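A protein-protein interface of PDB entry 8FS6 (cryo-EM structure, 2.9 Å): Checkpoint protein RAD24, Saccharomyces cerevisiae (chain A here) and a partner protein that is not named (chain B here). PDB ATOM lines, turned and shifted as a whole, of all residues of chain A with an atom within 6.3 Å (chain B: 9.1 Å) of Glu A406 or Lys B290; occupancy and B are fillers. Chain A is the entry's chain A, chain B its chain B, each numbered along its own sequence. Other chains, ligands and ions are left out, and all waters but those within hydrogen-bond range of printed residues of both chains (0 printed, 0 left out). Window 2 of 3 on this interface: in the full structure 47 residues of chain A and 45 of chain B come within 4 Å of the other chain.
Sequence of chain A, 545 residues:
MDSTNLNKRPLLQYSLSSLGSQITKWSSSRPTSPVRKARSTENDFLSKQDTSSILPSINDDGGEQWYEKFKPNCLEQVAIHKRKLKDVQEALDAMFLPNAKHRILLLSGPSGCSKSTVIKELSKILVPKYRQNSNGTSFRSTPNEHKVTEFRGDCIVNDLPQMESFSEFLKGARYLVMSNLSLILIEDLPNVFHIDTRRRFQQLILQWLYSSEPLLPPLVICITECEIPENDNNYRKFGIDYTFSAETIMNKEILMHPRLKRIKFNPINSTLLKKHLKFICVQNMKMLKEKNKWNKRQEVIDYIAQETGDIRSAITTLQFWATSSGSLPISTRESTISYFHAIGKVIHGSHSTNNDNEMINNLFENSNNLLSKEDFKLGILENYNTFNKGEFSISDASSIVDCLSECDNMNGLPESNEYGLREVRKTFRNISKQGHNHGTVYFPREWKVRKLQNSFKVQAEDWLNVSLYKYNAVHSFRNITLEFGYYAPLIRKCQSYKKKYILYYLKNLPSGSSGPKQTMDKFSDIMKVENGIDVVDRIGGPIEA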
ATOM      1  N   VAL A 401      40.361 -15.852  20.526  1.00  0.00           N
ATOM      2  CA  VAL A 401      41.028 -15.995  21.818  1.00  0.00           C
ATOM      3  C   VAL A 401      40.443 -15.094  22.901  1.00  0.00           C
ATOM      4  O   VAL A 401      40.404 -15.503  24.067  1.00  0.00           O
ATOM      5  CB  VAL A 401      42.544 -15.759  21.722  1.00  0.00           C
ATOM      6  CG1 VAL A 401      43.223 -16.323  22.945  1.00  0.00           C
ATOM      7  CG2 VAL A 401      43.109 -16.458  20.507  1.00  0.00           C
ATOM      8  N   ASP A 402      39.987 -13.882  22.573  1.00  0.00           N
ATOM      9  CA  ASP A 402      39.399 -13.048  23.616  1.00  0.00           C
ATOM     10  C   ASP A 402      38.088 -13.631  24.132  1.00  0.00           C
ATOM     11  O   ASP A 402      37.817 -13.557  25.335  1.00  0.00           O
ATOM     12  CB  ASP A 402      39.208 -11.609  23.115  1.00  0.00           C
ATOM     13  CG  ASP A 402      38.060 -11.464  22.131  1.00  0.00           C
ATOM     14  OD1 ASP A 402      37.688 -12.461  21.481  1.00  0.00           O
ATOM     15  OD2 ASP A 402      37.529 -10.342  22.007  1.00  0.00           O
ATOM     16  N   CYS A 403      37.280 -14.233  23.253  1.00  0.00           N
ATOM     17  CA  CYS A 403      36.085 -14.926  23.722  1.00  0.00           C
ATOM     18  C   CYS A 403      36.443 -16.162  24.537  1.00  0.00           C
ATOM     19  O   CYS A 403      35.799 -16.436  25.557  1.00  0.00           O
ATOM     20  CB  CYS A 403      35.191 -15.318  22.545  1.00  0.00           C
ATOM     21  SG  CYS A 403      35.531 -16.955  21.856  1.00  0.00           S
ATOM     22  N   LEU A 404      37.463 -16.917  24.112  1.00  0.00           N
ATOM     23  CA  LEU A 404      37.888 -18.074  24.893  1.00  0.00           C
ATOM     24  C   LEU A 404      38.426 -17.684  26.266  1.00  0.00           C
ATOM     25  O   LEU A 404      38.275 -18.454  27.219  1.00  0.00           O
ATOM     26  CB  LEU A 404      38.942 -18.875  24.128  1.00  0.00           C
ATOM     27  CG  LEU A 404      38.420 -19.759  22.994  1.00  0.00           C
ATOM     28  CD1 LEU A 404      39.571 -20.407  22.241  1.00  0.00           C
ATOM     29  CD2 LEU A 404      37.465 -20.814  23.532  1.00  0.00           C
ATOM     30  N   SER A 405      39.050 -16.512  26.383  1.00  0.00           N
ATOM     31  CA  SER A 405      39.507 -16.005  27.670  1.00  0.00           C
ATOM     32  C   SER A 405      38.369 -15.460  28.521  1.00  0.00           C
ATOM     33  O   SER A 405      38.391 -15.617  29.747  1.00  0.00           O
ATOM     34  CB  SER A 405      40.560 -14.911  27.465  1.00  0.00           C
ATOM     35  OG  SER A 405      39.989 -13.761  26.866  1.00  0.00           O
ATOM     36  N   GLU A 406      37.380 -14.813  27.898  1.00  0.00           N
ATOM     37  CA  GLU A 406      36.197 -14.367  28.622  1.00  0.00           C
ATOM     38  C   GLU A 406      35.370 -15.536  29.136  1.00  0.00           C
ATOM     39  O   GLU A 406      34.709 -15.404  30.172  1.00  0.00           O
ATOM     40  CB  GLU A 406      35.337 -13.477  27.722  1.00  0.00           C
ATOM     41  CG  GLU A 406      34.828 -12.212  28.392  1.00  0.00           C
ATOM     42  CD  GLU A 406      34.463 -11.134  27.391  1.00  0.00           C
ATOM     43  OE1 GLU A 406      34.625 -11.371  26.175  1.00  0.00           O
ATOM     44  OE2 GLU A 406      34.015 -10.051  27.819  1.00  0.00           O
ATOM     45  N   CYS A 407      35.388 -16.668  28.434  1.00  0.00           N
ATOM     46  CA  CYS A 407      34.691 -17.862  28.893  1.00  0.00           C
ATOM     47  C   CYS A 407      35.349 -18.496  30.111  1.00  0.00           C
ATOM     48  O   CYS A 407      34.663 -19.156  30.900  1.00  0.00           O
ATOM     49  CB  CYS A 407      34.616 -18.894  27.765  1.00  0.00           C
ATOM     50  SG  CYS A 407      33.501 -18.438  26.426  1.00  0.00           S
ATOM     51  N   ASP A 408      36.660 -18.314  30.279  1.00  0.00           N
ATOM     52  CA  ASP A 408      37.356 -18.896  31.420  1.00  0.00           C
ATOM     53  C   ASP A 408      36.993 -18.214  32.732  1.00  0.00           C
ATOM     54  O   ASP A 408      37.189 -18.808  33.798  1.00  0.00           O
ATOM     55  CB  ASP A 408      38.869 -18.831  31.203  1.00  0.00           C
ATOM     56  CG  ASP A 408      39.622 -19.849  32.036  1.00  0.00           C
ATOM     57  OD1 ASP A 408      39.524 -21.057  31.732  1.00  0.00           O
ATOM     58  OD2 ASP A 408      40.311 -19.442  32.994  1.00  0.00           O
ATOM     59  N   ASN A 409      36.473 -16.990  32.682  1.00  0.00           N
ATOM     60  CA  ASN A 409      36.071 -16.263  33.878  1.00  0.00           C
ATOM     61  C   ASN A 409      34.609 -16.476  34.242  1.00  0.00           C
ATOM     62  O   ASN A 409      34.143 -15.900  35.228  1.00  0.00           O
ATOM     63  CB  ASN A 409      36.342 -14.766  33.704  1.00  0.00           C
ATOM     64  CG  ASN A 409      37.819 -14.440  33.683  1.00  0.00           C
ATOM     65  OD1 ASN A 409      38.653 -15.293  33.378  1.00  0.00           O
ATOM     66  ND2 ASN A 409      38.154 -13.201  34.022  1.00  0.00           N
ATOM     67  N   MET A 410      33.879 -17.284  33.477  1.00  0.00           N
ATOM     68  CA  MET A 410      32.476 -17.557  33.756  1.00  0.00           C
ATOM     69  C   MET A 410      32.281 -18.721  34.717  1.00  0.00           C
ATOM     70  O   MET A 410      31.134 -19.083  35.002  1.00  0.00           O
ATOM     71  CB  MET A 410      31.723 -17.825  32.449  1.00  0.00           C
ATOM     72  CG  MET A 410      31.539 -16.588  31.583  1.00  0.00           C
ATOM     73  SD  MET A 410      29.973 -16.575  30.690  1.00  0.00           S
ATOM     74  CE  MET A 410      30.488 -15.888  29.118  1.00  0.00           C
ATOM     75  N   GLU A 415      26.365 -21.297  30.092  1.00  0.00           N
ATOM     76  CA  GLU A 415      26.357 -20.231  29.099  1.00  0.00           C
ATOM     77  C   GLU A 415      27.752 -19.875  28.601  1.00  0.00           C
ATOM     78  O   GLU A 415      27.873 -19.072  27.670  1.00  0.00           O
ATOM     79  CB  GLU A 415      25.683 -18.982  29.676  1.00  0.00           C
ATOM     80  CG  GLU A 415      24.246 -19.199  30.118  1.00  0.00           C
ATOM     81  CD  GLU A 415      24.124 -19.462  31.606  1.00  0.00           C
ATOM     82  OE1 GLU A 415      25.059 -20.053  32.186  1.00  0.00           O
ATOM     83  OE2 GLU A 415      23.092 -19.078  32.195  1.00  0.00           O
ATOM     84  N   SER A 416      28.802 -20.442  29.196  1.00  0.00           N
ATOM     85  CA  SER A 416      30.172 -20.162  28.785  1.00  0.00           C
ATOM     86  C   SER A 416      30.594 -21.010  27.589  1.00  0.00           C
ATOM     87  O   SER A 416      31.122 -20.481  26.606  1.00  0.00           O
ATOM     88  CB  SER A 416      31.129 -20.392  29.957  1.00  0.00           C
ATOM     89  OG  SER A 416      31.542 -21.746  30.019  1.00  0.00           O
ATOM     90  N   TYR A 419      28.807 -20.112  24.396  1.00  0.00           N
ATOM     91  CA  TYR A 419      29.293 -18.896  23.757  1.00  0.00           C
ATOM     92  C   TYR A 419      30.661 -19.102  23.119  1.00  0.00           C
ATOM     93  O   TYR A 419      30.906 -18.625  22.002  1.00  0.00           O
ATOM     94  CB  TYR A 419      29.352 -17.755  24.776  1.00  0.00           C
ATOM     95  CG  TYR A 419      30.114 -16.536  24.302  1.00  0.00           C
ATOM     96  CD1 TYR A 419      29.610 -15.726  23.294  1.00  0.00           C
ATOM     97  CD2 TYR A 419      31.333 -16.192  24.871  1.00  0.00           C
ATOM     98  CE1 TYR A 419      30.302 -14.611  22.861  1.00  0.00           C
ATOM     99  CE2 TYR A 419      32.033 -15.079  24.444  1.00  0.00           C
ATOM    100  CZ  TYR A 419      31.512 -14.293  23.439  1.00  0.00           C
ATOM    101  OH  TYR A 419      32.204 -13.183  23.011  1.00  0.00           O
ATOM    102  N   VAL B 267      16.685 -16.014  34.525  1.00  0.00           N
ATOM    103  CA  VAL B 267      17.902 -16.128  33.725  1.00  0.00           C
ATOM    104  C   VAL B 267      18.037 -17.527  33.128  1.00  0.00           C
ATOM    105  O   VAL B 267      18.415 -17.687  31.957  1.00  0.00           O
ATOM    106  CB  VAL B 267      19.130 -15.746  34.573  1.00  0.00           C
ATOM    107  CG1 VAL B 267      20.412 -16.088  33.841  1.00  0.00           C
ATOM    108  CG2 VAL B 267      19.092 -14.268  34.909  1.00  0.00           C
ATOM    109  N   PHE B 271      18.141 -18.308  29.080  1.00  0.00           N
ATOM    110  CA  PHE B 271      19.170 -19.036  28.341  1.00  0.00           C
ATOM    111  C   PHE B 271      18.552 -20.092  27.429  1.00  0.00           C
ATOM    112  O   PHE B 271      18.933 -20.215  26.257  1.00  0.00           O
ATOM    113  CB  PHE B 271      20.160 -19.676  29.313  1.00  0.00           C
ATOM    114  CG  PHE B 271      21.242 -20.472  28.642  1.00  0.00           C
ATOM    115  CD1 PHE B 271      21.935 -19.952  27.560  1.00  0.00           C
ATOM    116  CD2 PHE B 271      21.572 -21.738  29.096  1.00  0.00           C
ATOM    117  CE1 PHE B 271      22.933 -20.681  26.943  1.00  0.00           C
ATOM    118  CE2 PHE B 271      22.570 -22.471  28.483  1.00  0.00           C
ATOM    119  CZ  PHE B 271      23.250 -21.942  27.405  1.00  0.00           C
ATOM    120  N   THR B 274      16.780 -18.381  24.516  1.00  0.00           N
ATOM    121  CA  THR B 274      17.762 -17.881  23.560  1.00  0.00           C
ATOM    122  C   THR B 274      18.338 -19.012  22.716  1.00  0.00           C
ATOM    123  O   THR B 274      18.562 -18.845  21.512  1.00  0.00           O
ATOM    124  CB  THR B 274      18.874 -17.137  24.303  1.00  0.00           C
ATOM    125  OG1 THR B 274      18.330 -15.969  24.930  1.00  0.00           O
ATOM    126  CG2 THR B 274      19.979 -16.716  23.348  1.00  0.00           C
ATOM    127  N   GLU B 282      23.022 -15.309  14.258  1.00  0.00           N
ATOM    128  CA  GLU B 282      23.827 -16.115  15.171  1.00  0.00           C
ATOM    129  C   GLU B 282      24.759 -15.261  16.022  1.00  0.00           C
ATOM    130  O   GLU B 282      25.001 -15.592  17.188  1.00  0.00           O
ATOM    131  CB  GLU B 282      24.623 -17.158  14.386  1.00  0.00           C
ATOM    132  CG  GLU B 282      23.759 -18.057  13.513  1.00  0.00           C
ATOM    133  CD  GLU B 282      22.913 -19.024  14.321  1.00  0.00           C
ATOM    134  OE1 GLU B 282      23.257 -19.289  15.493  1.00  0.00           O
ATOM    135  OE2 GLU B 282      21.900 -19.518  13.784  1.00  0.00           O
ATOM    136  N   SER B 283      25.300 -14.175  15.461  1.00  0.00           N
ATOM    137  CA  SER B 283      26.115 -13.266  16.262  1.00  0.00           C
ATOM    138  C   SER B 283      25.291 -12.634  17.378  1.00  0.00           C
ATOM    139  O   SER B 283      25.744 -12.546  18.527  1.00  0.00           O
ATOM    140  CB  SER B 283      26.731 -12.189  15.371  1.00  0.00           C
ATOM    141  OG  SER B 283      25.733 -11.340  14.831  1.00  0.00           O
ATOM    142  N   VAL B 284      24.068 -12.209  17.056  1.00  0.00           N
ATOM    143  CA  VAL B 284      23.169 -11.659  18.066  1.00  0.00           C
ATOM    144  C   VAL B 284      22.849 -12.710  19.121  1.00  0.00           C
ATOM    145  O   VAL B 284      22.828 -12.416  20.322  1.00  0.00           O
ATOM    146  CB  VAL B 284      21.897 -11.113  17.391  1.00  0.00           C
ATOM    147  CG1 VAL B 284      20.757 -10.984  18.390  1.00  0.00           C
ATOM    148  CG2 VAL B 284      22.183  -9.774  16.728  1.00  0.00           C
ATOM    149  N   ARG B 285      22.613 -13.954  18.694  1.00  0.00           N
ATOM    150  CA  ARG B 285      22.282 -15.018  19.639  1.00  0.00           C
ATOM    151  C   ARG B 285      23.442 -15.318  20.582  1.00  0.00           C
ATOM    152  O   ARG B 285      23.237 -15.477  21.790  1.00  0.00           O
ATOM    153  CB  ARG B 285      21.867 -16.278  18.881  1.00  0.00           C
ATOM    154  CG  ARG B 285      21.453 -17.431  19.781  1.00  0.00           C
ATOM    155  CD  ARG B 285      21.494 -18.752  19.033  1.00  0.00           C
ATOM    156  NE  ARG B 285      20.890 -18.645  17.712  1.00  0.00           N
ATOM    157  CZ  ARG B 285      19.588 -18.720  17.474  1.00  0.00           C
ATOM    158  NH1 ARG B 285      18.717 -18.906  18.452  1.00  0.00           N
ATOM    159  NH2 ARG B 285      19.148 -18.606  16.224  1.00  0.00           N
ATOM    160  N   LEU B 286      24.670 -15.399  20.057  1.00  0.00           N
ATOM    161  CA  LEU B 286      25.809 -15.682  20.925  1.00  0.00           C
ATOM    162  C   LEU B 286      26.110 -14.513  21.854  1.00  0.00           C
ATOM    163  O   LEU B 286      26.483 -14.727  23.016  1.00  0.00           O
ATOM    164  CB  LEU B 286      27.043 -16.055  20.097  1.00  0.00           C
ATOM    165  CG  LEU B 286      27.653 -15.091  19.075  1.00  0.00           C
ATOM    166  CD1 LEU B 286      28.744 -14.224  19.689  1.00  0.00           C
ATOM    167  CD2 LEU B 286      28.204 -15.872  17.893  1.00  0.00           C
ATOM    168  N   GLU B 287      25.944 -13.276  21.378  1.00  0.00           N
ATOM    169  CA  GLU B 287      26.105 -12.130  22.265  1.00  0.00           C
ATOM    170  C   GLU B 287      25.052 -12.137  23.369  1.00  0.00           C
ATOM    171  O   GLU B 287      25.355 -11.819  24.525  1.00  0.00           O
ATOM    172  CB  GLU B 287      26.049 -10.832  21.460  1.00  0.00           C
ATOM    173  CG  GLU B 287      27.323 -10.522  20.692  1.00  0.00           C
ATOM    174  CD  GLU B 287      28.508 -10.263  21.604  1.00  0.00           C
ATOM    175  OE1 GLU B 287      28.304  -9.709  22.705  1.00  0.00           O
ATOM    176  OE2 GLU B 287      29.644 -10.613  21.220  1.00  0.00           O
ATOM    177  N   MET B 288      23.810 -12.504  23.033  1.00  0.00           N
ATOM    178  CA  MET B 288      22.765 -12.607  24.046  1.00  0.00           C
ATOM    179  C   MET B 288      23.078 -13.704  25.054  1.00  0.00           C
ATOM    180  O   MET B 288      22.820 -13.545  26.252  1.00  0.00           O
ATOM    181  CB  MET B 288      21.409 -12.853  23.381  1.00  0.00           C
ATOM    182  CG  MET B 288      20.615 -11.584  23.121  1.00  0.00           C
ATOM    183  SD  MET B 288      19.200 -11.798  22.023  1.00  0.00           S
ATOM    184  CE  MET B 288      18.652 -13.441  22.470  1.00  0.00           C
ATOM    185  N   ILE B 289      23.630 -14.826  24.585  1.00  0.00           N
ATOM    186  CA  ILE B 289      24.049 -15.892  25.492  1.00  0.00           C
ATOM    187  C   ILE B 289      25.122 -15.387  26.447  1.00  0.00           C
ATOM    188  O   ILE B 289      25.079 -15.656  27.655  1.00  0.00           O
ATOM    189  CB  ILE B 289      24.535 -17.115  24.691  1.00  0.00           C
ATOM    190  CG1 ILE B 289      23.355 -17.826  24.028  1.00  0.00           C
ATOM    191  CG2 ILE B 289      25.300 -18.080  25.585  1.00  0.00           C
ATOM    192  CD1 ILE B 289      23.753 -19.030  23.206  1.00  0.00           C
ATOM    193  N   LYS B 290      26.101 -14.644  25.922  1.00  0.00           N
ATOM    194  CA  LYS B 290      27.162 -14.105  26.770  1.00  0.00           C
ATOM    195  C   LYS B 290      26.607 -13.137  27.810  1.00  0.00           C
ATOM    196  O   LYS B 290      26.989 -13.190  28.986  1.00  0.00           O
ATOM    197  CB  LYS B 290      28.220 -13.417  25.907  1.00  0.00           C
ATOM    198  CG  LYS B 290      29.214 -12.575  26.692  1.00  0.00           C
ATOM    199  CD  LYS B 290      30.108 -11.768  25.766  1.00  0.00           C
ATOM    200  CE  LYS B 290      30.717 -10.577  26.489  1.00  0.00           C
ATOM    201  NZ  LYS B 290      31.314  -9.597  25.542  1.00  0.00           N
ATOM    202  N   GLU B 291      25.698 -12.248  27.398  1.00  0.00           N
ATOM    203  CA  GLU B 291      25.124 -11.294  28.341  1.00  0.00           C
ATOM    204  C   GLU B 291      24.225 -11.965  29.372  1.00  0.00           C
ATOM    205  O   GLU B 291      24.152 -11.493  30.512  1.00  0.00           O
ATOM    206  CB  GLU B 291      24.343 -10.204  27.603  1.00  0.00           C
ATOM    207  CG  GLU B 291      25.144  -9.443  26.549  1.00  0.00           C
ATOM    208  CD  GLU B 291      26.204  -8.524  27.133  1.00  0.00           C
ATOM    209  OE1 GLU B 291      26.250  -8.356  28.370  1.00  0.00           O
ATOM    210  OE2 GLU B 291      26.997  -7.964  26.348  1.00  0.00           O
ATOM    211  N   ILE B 292      23.535 -13.044  28.999  1.00  0.00           N
ATOM    212  CA  ILE B 292      22.736 -13.790  29.967  1.00  0.00           C
ATOM    213  C   ILE B 292      23.635 -14.506  30.968  1.00  0.00           C
ATOM    214  O   ILE B 292      23.357 -14.515  32.171  1.00  0.00           O
ATOM    215  CB  ILE B 292      21.795 -14.764  29.234  1.00  0.00           C
ATOM    216  CG1 ILE B 292      20.643 -13.996  28.582  1.00  0.00           C
ATOM    217  CG2 ILE B 292      21.251 -15.818  30.185  1.00  0.00           C
ATOM    218  CD1 ILE B 292      19.761 -14.850  27.705  1.00  0.00           C
ATOM    219  N   GLY B 293      24.731 -15.104  30.495  1.00  0.00           N
ATOM    220  CA  GLY B 293      25.671 -15.755  31.392  1.00  0.00           C
ATOM    221  C   GLY B 293      26.378 -14.810  32.342  1.00  0.00           C
ATOM    222  O   GLY B 293      26.624 -15.175  33.498  1.00  0.00           O
ATOM    223  N   LEU B 294      26.712 -13.602  31.879  1.00  0.00           N
ATOM    224  CA  LEU B 294      27.336 -12.620  32.758  1.00  0.00           C
ATOM    225  C   LEU B 294      26.410 -12.199  33.893  1.00  0.00           C
ATOM    226  O   LEU B 294      26.879 -11.956  35.011  1.00  0.00           O
ATOM    227  CB  LEU B 294      27.780 -11.398  31.954  1.00  0.00           C
ATOM    228  CG  LEU B 294      28.987 -11.615  31.038  1.00  0.00           C
ATOM    229  CD1 LEU B 294      29.353 -10.331  30.311  1.00  0.00           C
ATOM    230  CD2 LEU B 294      30.174 -12.148  31.825  1.00  0.00           C
ATOM    231  N   THR B 295      25.105 -12.103  33.630  1.00  0.00           N
ATOM    232  CA  THR B 295      24.143 -11.827  34.692  1.00  0.00           C
ATOM    233  C   THR B 295      23.896 -13.055  35.563  1.00  0.00           C
ATOM    234  O   THR B 295      23.646 -12.917  36.766  1.00  0.00           O
ATOM    235  CB  THR B 295      22.827 -11.332  34.092  1.00  0.00           C
ATOM    236  OG1 THR B 295      23.101 -10.334  33.101  1.00  0.00           O
ATOM    237  CG2 THR B 295      21.937 -10.726  35.169  1.00  0.00           C
ATOM    238  N   HIS B 296      23.956 -14.251  34.972  1.00  0.00           N
ATOM    239  CA  HIS B 296      23.819 -15.480  35.747  1.00  0.00           C
ATOM    240  C   HIS B 296      24.928 -15.600  36.782  1.00  0.00           C
ATOM    241  O   HIS B 296      24.684 -16.007  37.922  1.00  0.00           O
ATOM    242  CB  HIS B 296      23.829 -16.690  34.812  1.00  0.00           C
ATOM    243  CG  HIS B 296      23.438 -17.974  35.475  1.00  0.00           C
ATOM    244  ND1 HIS B 296      24.324 -18.736  36.204  1.00  0.00           N
ATOM    245  CD2 HIS B 296      22.256 -18.634  35.510  1.00  0.00           C
ATOM    246  CE1 HIS B 296      23.705 -19.809  36.664  1.00  0.00           C
ATOM    247  NE2 HIS B 296      22.449 -19.771  36.256  1.00  0.00           N
ATOM    248  N   MET B 297      26.157 -15.250  36.395  1.00  0.00           N
ATOM    249  CA  MET B 297      27.267 -15.265  37.343  1.00  0.00           C
ATOM    250  C   MET B 297      27.045 -14.286  38.491  1.00  0.00           C
ATOM    251  O   MET B 297      27.294 -14.628  39.653  1.00  0.00           O
ATOM    252  CB  MET B 297      28.575 -14.942  36.623  1.00  0.00           C
ATOM    253  CG  MET B 297      29.738 -15.833  37.016  1.00  0.00           C
ATOM    254  SD  MET B 297      31.329 -15.154  36.510  1.00  0.00           S
ATOM    255  CE  MET B 297      30.872 -14.254  35.030  1.00  0.00           C
ATOM    256  N   MET B 312      20.707  -6.474  32.061  1.00  0.00           N
ATOM    257  CA  MET B 312      20.829  -7.542  31.073  1.00  0.00           C
ATOM    258  C   MET B 312      19.933  -7.280  29.870  1.00  0.00           C
ATOM    259  O   MET B 312      20.356  -7.451  28.720  1.00  0.00           O
ATOM    260  CB  MET B 312      20.496  -8.889  31.717  1.00  0.00           C
ATOM    261  CG  MET B 312      19.864  -9.905  30.776  1.00  0.00           C
ATOM    262  SD  MET B 312      19.328 -11.402  31.624  1.00  0.00           S
ATOM    263  CE  MET B 312      17.549 -11.272  31.452  1.00  0.00           C
ATOM    264  N   LYS B 315      21.495  -4.448  27.809  1.00  0.00           N
ATOM    265  CA  LYS B 315      22.606  -4.922  26.990  1.00  0.00           C
ATOM    266  C   LYS B 315      22.128  -5.784  25.827  1.00  0.00           C
ATOM    267  O   LYS B 315      22.719  -5.737  24.740  1.00  0.00           O
ATOM    268  CB  LYS B 315      23.603  -5.693  27.857  1.00  0.00           C
ATOM    269  CG  LYS B 315      24.401  -4.800  28.796  1.00  0.00           C
ATOM    270  CD  LYS B 315      25.339  -5.599  29.680  1.00  0.00           C
ATOM    271  CE  LYS B 315      26.228  -4.684  30.506  1.00  0.00           C
ATOM    272  NZ  LYS B 315      27.260  -5.445  31.262  1.00  0.00           N
ATOM    273  N   ILE B 316      21.064  -6.565  26.032  1.00  0.00           N
ATOM    274  CA  ILE B 316      20.477  -7.325  24.932  1.00  0.00           C
ATOM    275  C   ILE B 316      19.939  -6.384  23.859  1.00  0.00           C
ATOM    276  O   ILE B 316      20.137  -6.608  22.660  1.00  0.00           O
ATOM    277  CB  ILE B 316      19.389  -8.275  25.467  1.00  0.00           C
ATOM    278  CG1 ILE B 316      20.035  -9.471  26.170  1.00  0.00           C
ATOM    279  CG2 ILE B 316      18.475  -8.746  24.346  1.00  0.00           C
ATOM    280  CD1 ILE B 316      19.055 -10.351  26.906  1.00  0.00           C
ATOM    281  N   LEU B 319      22.933  -4.899  21.942  1.00  0.00           N
ATOM    282  CA  LEU B 319      23.430  -5.818  20.927  1.00  0.00           C
ATOM    283  C   LEU B 319      22.418  -6.025  19.807  1.00  0.00           C
ATOM    284  O   LEU B 319      22.804  -6.412  18.700  1.00  0.00           O
ATOM    285  CB  LEU B 319      23.832  -7.141  21.593  1.00  0.00           C
ATOM    286  CG  LEU B 319      22.825  -8.156  22.164  1.00  0.00           C
ATOM    287  CD1 LEU B 319      21.982  -8.909  21.124  1.00  0.00           C
ATOM    288  CD2 LEU B 319      23.499  -9.111  23.135  1.00  0.00           C
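The side-chain carboxylate (OE2) of Glu A406 is in salt-bridge range of the side-chain amino group (NZ) of Lys B290. The backbone carbonyl oxygen of Asn A409 lies close to the side-chain sulfur of Met B297, 3.2 Å away.
Among the printed residues, merely in contact across the chains: Met A410 with Met B297, Glu A415 with Phe B271, Glu A415 with Ile B289, Glu A415 with Gly B293, Glu A415 with His B296, Tyr A419 with Leu B286 and Tyr A419 with Lys B290.
Of chain A, only Glu A406 (3.6 Å) and Tyr A419 (3.7 Å) come within 4 Å of Lys B290. No residue of chain B comes within 4 Å of Ser A405. Printed residues of chain B within 4 Å of Glu A415: Phe B271, Ile B289, Gly B293 and His B296. Printed residues of chain A within 4 Å of Met B297: Asn A409 and Met A410. Printed residues of chain A within 4 Å of Leu B286: Tyr A419 (3.3 Å). Cys A403 touches none of the printed residues of chain B. Asp A402 touches none of the printed residues of chain B. The nearest printed residue of chain A that does not touch Gly B293 is Met A410 (4.3 Å).
Hydrophobic or aromatic side chains of chain B within 4 Å of the printed part of chain A: Phe B271, Leu B286, Ile B289, His B296 and Met B297. Of the 13 printed residues of chain A, 5 touch a printed residue of chain B. Printed residues of chain A that touch a printed residue of chain B: Glu A406, Asn A409, Met A410, Glu A415 and Tyr A419. Hydrophobic or aromatic side chains of chain A within 4 Å of the printed part of chain B: Tyr A419. Among the printed residues, 9 pairs touch across the chains.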
